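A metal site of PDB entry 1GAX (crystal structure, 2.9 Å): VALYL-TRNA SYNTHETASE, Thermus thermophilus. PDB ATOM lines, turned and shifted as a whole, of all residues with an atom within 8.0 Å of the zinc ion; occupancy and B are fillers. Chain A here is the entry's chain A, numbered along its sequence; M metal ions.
The backbone NH of Cys 344 is in hydrogen-bond range of the backbone carbonyl oxygen of Thr 349, 2.7 Å away.
SG of Cys 347 lies close to N of Thr 349 (3.5 Å).
The backbone carbonyl oxygen (O) of Thr 181 sits at hydrogen-bond distance from the backbone NH (N) of Cys 176, 3.2 Å away.
SG of Cys 176 sits close to N of Arg 178, at 3.1 Å.
CG of Arg 178 touches the zinc ion, 3.4 Å away.
The zinc ion is bound by SG of Cys 344 (2.5 Å), SG of Cys 347 (2.5 Å), SG of Cys 176 (2.6 Å) and SG of Cys 179 (2.6 Å).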
ATOM      1  N   ILE A  85      13.825  -1.716   7.486  1.00  0.00           N
ATOM      2  CA  ILE A  85      12.384  -1.762   7.201  1.00  0.00           C
ATOM      3  C   ILE A  85      11.840  -3.164   7.497  1.00  0.00           C
ATOM      4  O   ILE A  85      10.804  -3.326   8.157  1.00  0.00           O
ATOM      5  CB  ILE A  85      12.081  -1.388   5.699  1.00  0.00           C
ATOM      6  CG1 ILE A  85      10.607  -1.644   5.376  1.00  0.00           C
ATOM      7  CG2 ILE A  85      12.914  -2.245   4.732  1.00  0.00           C
ATOM      8  CD1 ILE A  85       9.652  -0.964   6.308  1.00  0.00           C
ATOM      9  N   VAL A  89       9.064  -4.255  10.422  1.00  0.00           N
ATOM     10  CA  VAL A  89       7.777  -4.880  10.192  1.00  0.00           C
ATOM     11  C   VAL A  89       7.603  -6.086  11.100  1.00  0.00           C
ATOM     12  O   VAL A  89       6.703  -6.130  11.923  1.00  0.00           O
ATOM     13  CB  VAL A  89       7.659  -5.381   8.759  1.00  0.00           C
ATOM     14  CG1 VAL A  89       6.219  -5.749   8.466  1.00  0.00           C
ATOM     15  CG2 VAL A  89       8.175  -4.332   7.799  1.00  0.00           C
ATOM     16  N   GLU A  92       7.057  -5.159  14.686  1.00  0.00           N
ATOM     17  CA  GLU A  92       5.863  -4.314  14.706  1.00  0.00           C
ATOM     18  C   GLU A  92       4.663  -5.239  14.541  1.00  0.00           C
ATOM     19  O   GLU A  92       3.715  -5.207  15.324  1.00  0.00           O
ATOM     20  CB  GLU A  92       5.934  -3.320  13.541  1.00  0.00           C
ATOM     21  CG  GLU A  92       5.053  -2.091  13.634  1.00  0.00           C
ATOM     22  CD  GLU A  92       5.377  -1.091  12.537  1.00  0.00           C
ATOM     23  OE1 GLU A  92       5.042  -1.360  11.359  1.00  0.00           O
ATOM     24  OE2 GLU A  92       5.976  -0.046  12.853  1.00  0.00           O
ATOM     25  N   TRP A 175       6.317   7.087  -0.955  1.00  0.00           N
ATOM     26  CA  TRP A 175       5.993   7.001   0.460  1.00  0.00           C
ATOM     27  C   TRP A 175       4.873   6.050   0.862  1.00  0.00           C
ATOM     28  O   TRP A 175       3.781   6.086   0.301  1.00  0.00           O
ATOM     29  CB  TRP A 175       5.691   8.419   0.980  1.00  0.00           C
ATOM     30  CG  TRP A 175       4.897   8.497   2.263  1.00  0.00           C
ATOM     31  CD1 TRP A 175       3.550   8.292   2.423  1.00  0.00           C
ATOM     32  CD2 TRP A 175       5.416   8.767   3.569  1.00  0.00           C
ATOM     33  NE1 TRP A 175       3.196   8.415   3.747  1.00  0.00           N
ATOM     34  CE2 TRP A 175       4.319   8.703   4.473  1.00  0.00           C
ATOM     35  CE3 TRP A 175       6.686   9.052   4.068  1.00  0.00           C
ATOM     36  CZ2 TRP A 175       4.472   8.908   5.850  1.00  0.00           C
ATOM     37  CZ3 TRP A 175       6.845   9.258   5.436  1.00  0.00           C
ATOM     38  CH2 TRP A 175       5.738   9.186   6.308  1.00  0.00           C
ATOM     39  N   CYS A 176       5.138   5.209   1.855  1.00  0.00           N
ATOM     40  CA  CYS A 176       4.140   4.280   2.355  1.00  0.00           C
ATOM     41  C   CYS A 176       3.546   4.830   3.638  1.00  0.00           C
ATOM     42  O   CYS A 176       4.250   4.985   4.638  1.00  0.00           O
ATOM     43  CB  CYS A 176       4.742   2.903   2.656  1.00  0.00           C
ATOM     44  SG  CYS A 176       3.666   1.853   3.716  1.00  0.00           S
ATOM     45  N   PRO A 177       2.249   5.123   3.623  1.00  0.00           N
ATOM     46  CA  PRO A 177       1.558   5.666   4.801  1.00  0.00           C
ATOM     47  C   PRO A 177       1.252   4.606   5.859  1.00  0.00           C
ATOM     48  O   PRO A 177       0.578   4.902   6.850  1.00  0.00           O
ATOM     49  CB  PRO A 177       0.305   6.268   4.203  1.00  0.00           C
ATOM     50  CG  PRO A 177       0.011   5.317   3.080  1.00  0.00           C
ATOM     51  CD  PRO A 177       1.369   5.135   2.451  1.00  0.00           C
ATOM     52  N   ARG A 178       1.735   3.386   5.648  1.00  0.00           N
ATOM     53  CA  ARG A 178       1.529   2.307   6.616  1.00  0.00           C
ATOM     54  C   ARG A 178       2.719   2.292   7.576  1.00  0.00           C
ATOM     55  O   ARG A 178       2.567   2.417   8.796  1.00  0.00           O
ATOM     56  CB  ARG A 178       1.447   0.943   5.894  1.00  0.00           C
ATOM     57  CG  ARG A 178       2.410  -0.158   6.403  1.00  0.00           C
ATOM     58  CD  ARG A 178       2.095  -0.691   7.807  1.00  0.00           C
ATOM     59  NE  ARG A 178       0.983  -1.635   7.837  1.00  0.00           N
ATOM     60  CZ  ARG A 178      -0.290  -1.340   7.582  1.00  0.00           C
ATOM     61  NH1 ARG A 178      -0.645  -0.101   7.248  1.00  0.00           N
ATOM     62  NH2 ARG A 178      -1.226  -2.284   7.648  1.00  0.00           N
ATOM     63  N   CYS A 179       3.893   2.165   6.992  1.00  0.00           N
ATOM     64  CA  CYS A 179       5.141   2.121   7.735  1.00  0.00           C
ATOM     65  C   CYS A 179       5.642   3.527   8.019  1.00  0.00           C
ATOM     66  O   CYS A 179       6.619   3.717   8.735  1.00  0.00           O
ATOM     67  CB  CYS A 179       6.167   1.318   6.930  1.00  0.00           C
ATOM     68  SG  CYS A 179       5.564  -0.321   6.450  1.00  0.00           S
ATOM     69  N   GLU A 180       4.959   4.519   7.453  1.00  0.00           N
ATOM     70  CA  GLU A 180       5.335   5.911   7.649  1.00  0.00           C
ATOM     71  C   GLU A 180       6.825   6.051   7.353  1.00  0.00           C
ATOM     72  O   GLU A 180       7.642   6.227   8.262  1.00  0.00           O
ATOM     73  CB  GLU A 180       5.034   6.322   9.090  1.00  0.00           C
ATOM     74  CG  GLU A 180       3.556   6.225   9.447  1.00  0.00           C
ATOM     75  CD  GLU A 180       3.292   6.123  10.940  1.00  0.00           C
ATOM     76  OE1 GLU A 180       3.866   6.907  11.708  1.00  0.00           O
ATOM     77  OE2 GLU A 180       2.486   5.268  11.335  1.00  0.00           O
ATOM     78  N   THR A 181       7.192   5.949   6.089  1.00  0.00           N
ATOM     79  CA  THR A 181       8.589   6.054   5.701  1.00  0.00           C
ATOM     80  C   THR A 181       8.749   6.040   4.201  1.00  0.00           C
ATOM     81  O   THR A 181       7.905   5.532   3.483  1.00  0.00           O
ATOM     82  CB  THR A 181       9.385   4.885   6.199  1.00  0.00           C
ATOM     83  OG1 THR A 181      10.615   4.820   5.464  1.00  0.00           O
ATOM     84  CG2 THR A 181       8.605   3.588   5.973  1.00  0.00           C
ATOM     85  N   LEU A 183      10.542   4.812   0.681  1.00  0.00           N
ATOM     86  CA  LEU A 183      11.125   3.578   0.161  1.00  0.00           C
ATOM     87  C   LEU A 183      11.953   3.947  -1.055  1.00  0.00           C
ATOM     88  O   LEU A 183      11.976   5.112  -1.462  1.00  0.00           O
ATOM     89  CB  LEU A 183      10.053   2.590  -0.297  1.00  0.00           C
ATOM     90  CG  LEU A 183       9.127   1.875   0.695  1.00  0.00           C
ATOM     91  CD1 LEU A 183       8.321   2.887   1.496  1.00  0.00           C
ATOM     92  CD2 LEU A 183       8.191   0.950  -0.079  1.00  0.00           C
ATOM     93  N   GLU A 187      12.653  -0.960  -3.729  1.00  0.00           N
ATOM     94  CA  GLU A 187      11.883  -1.466  -2.603  1.00  0.00           C
ATOM     95  C   GLU A 187      10.382  -1.428  -2.802  1.00  0.00           C
ATOM     96  O   GLU A 187       9.630  -1.893  -1.954  1.00  0.00           O
ATOM     97  CB  GLU A 187      12.237  -0.699  -1.330  1.00  0.00           C
ATOM     98  CG  GLU A 187      13.665  -0.894  -0.876  1.00  0.00           C
ATOM     99  CD  GLU A 187      13.943  -0.309   0.492  1.00  0.00           C
ATOM    100  OE1 GLU A 187      13.343  -0.767   1.483  1.00  0.00           O
ATOM    101  OE2 GLU A 187      14.773   0.616   0.570  1.00  0.00           O
ATOM    102  N   THR A 343       2.894  -0.645  -5.002  1.00  0.00           N
ATOM    103  CA  THR A 343       2.682  -0.983  -3.598  1.00  0.00           C
ATOM    104  C   THR A 343       3.956  -1.145  -2.797  1.00  0.00           C
ATOM    105  O   THR A 343       5.043  -1.303  -3.357  1.00  0.00           O
ATOM    106  CB  THR A 343       1.858  -2.271  -3.465  1.00  0.00           C
ATOM    107  OG1 THR A 343       2.515  -3.323  -4.177  1.00  0.00           O
ATOM    108  CG2 THR A 343       0.468  -2.068  -4.051  1.00  0.00           C
ATOM    109  N   CYS A 344       3.811  -1.114  -1.469  1.00  0.00           N
ATOM    110  CA  CYS A 344       4.959  -1.271  -0.572  1.00  0.00           C
ATOM    111  C   CYS A 344       5.354  -2.738  -0.506  1.00  0.00           C
ATOM    112  O   CYS A 344       4.626  -3.558   0.067  1.00  0.00           O
ATOM    113  CB  CYS A 344       4.613  -0.775   0.831  1.00  0.00           C
ATOM    114  SG  CYS A 344       6.050  -0.742   1.905  1.00  0.00           S
ATOM    115  N   SER A 345       6.513  -3.054  -1.076  1.00  0.00           N
ATOM    116  CA  SER A 345       6.982  -4.434  -1.124  1.00  0.00           C
ATOM    117  C   SER A 345       6.940  -5.153   0.226  1.00  0.00           C
ATOM    118  O   SER A 345       6.695  -6.364   0.279  1.00  0.00           O
ATOM    119  CB  SER A 345       8.406  -4.509  -1.676  1.00  0.00           C
ATOM    120  OG  SER A 345       9.368  -4.288  -0.663  1.00  0.00           O
ATOM    121  N   ARG A 346       7.159  -4.432   1.317  1.00  0.00           N
ATOM    122  CA  ARG A 346       7.171  -5.075   2.611  1.00  0.00           C
ATOM    123  C   ARG A 346       5.941  -4.941   3.510  1.00  0.00           C
ATOM    124  O   ARG A 346       5.974  -5.366   4.663  1.00  0.00           O
ATOM    125  CB  ARG A 346       8.434  -4.671   3.370  1.00  0.00           C
ATOM    126  CG  ARG A 346       8.919  -5.740   4.330  1.00  0.00           C
ATOM    127  CD  ARG A 346      10.432  -5.908   4.333  1.00  0.00           C
ATOM    128  NE  ARG A 346      11.002  -6.339   3.054  1.00  0.00           N
ATOM    129  CZ  ARG A 346      11.378  -5.522   2.077  1.00  0.00           C
ATOM    130  NH1 ARG A 346      11.252  -4.211   2.213  1.00  0.00           N
ATOM    131  NH2 ARG A 346      11.910  -6.015   0.962  1.00  0.00           N
ATOM    132  N   CYS A 347       4.858  -4.355   3.004  1.00  0.00           N
ATOM    133  CA  CYS A 347       3.642  -4.231   3.814  1.00  0.00           C
ATOM    134  C   CYS A 347       2.391  -4.344   2.973  1.00  0.00           C
ATOM    135  O   CYS A 347       1.281  -4.450   3.512  1.00  0.00           O
ATOM    136  CB  CYS A 347       3.601  -2.899   4.570  1.00  0.00           C
ATOM    137  SG  CYS A 347       2.544  -1.622   3.836  1.00  0.00           S
ATOM    138  N   GLY A 348       2.557  -4.307   1.652  1.00  0.00           N
ATOM    139  CA  GLY A 348       1.409  -4.424   0.774  1.00  0.00           C
ATOM    140  C   GLY A 348       0.788  -3.113   0.321  1.00  0.00           C
ATOM    141  O   GLY A 348       0.808  -2.805  -0.877  1.00  0.00           O
ATOM    142  N   THR A 349       0.224  -2.349   1.261  1.00  0.00           N
ATOM    143  CA  THR A 349      -0.404  -1.063   0.960  1.00  0.00           C
ATOM    144  C   THR A 349       0.241  -0.353  -0.239  1.00  0.00           C
ATOM    145  O   THR A 349       1.465  -0.358  -0.401  1.00  0.00           O
ATOM    146  CB  THR A 349      -0.324  -0.097   2.178  1.00  0.00           C
ATOM    147  OG1 THR A 349      -0.936  -0.701   3.322  1.00  0.00           O
ATOM    148  CG2 THR A 349      -1.014   1.214   1.872  1.00  0.00           C
ATOM    149  N   PRO A 350      -0.591   0.257  -1.106  1.00  0.00           N
ATOM    150  CA  PRO A 350      -0.055   0.954  -2.272  1.00  0.00           C
ATOM    151  C   PRO A 350       0.634   2.229  -1.805  1.00  0.00           C
ATOM    152  O   PRO A 350       0.143   2.912  -0.905  1.00  0.00           O
ATOM    153  CB  PRO A 350      -1.293   1.234  -3.101  1.00  0.00           C
ATOM    154  CG  PRO A 350      -2.327   1.489  -2.046  1.00  0.00           C
ATOM    155  CD  PRO A 350      -2.051   0.375  -1.051  1.00  0.00           C
ATOM    156  N   ILE A 351       1.779   2.531  -2.403  1.00  0.00           N
ATOM    157  CA  ILE A 351       2.559   3.698  -2.051  1.00  0.00           C
ATOM    158  C   ILE A 351       1.793   5.015  -2.153  1.00  0.00           C
ATOM    159  O   ILE A 351       0.616   5.116  -1.793  1.00  0.00           O
ATOM    160  CB  ILE A 351       3.820   3.801  -2.924  1.00  0.00           C
ATOM    161  CG1 ILE A 351       3.416   3.856  -4.396  1.00  0.00           C
ATOM    162  CG2 ILE A 351       4.737   2.634  -2.671  1.00  0.00           C
ATOM    163  CD1 ILE A 351       4.556   4.191  -5.326  1.00  0.00           C
HETATM  164 ZN    ZN M   1       4.725  -0.491   3.952  1.00  0.00          ZN
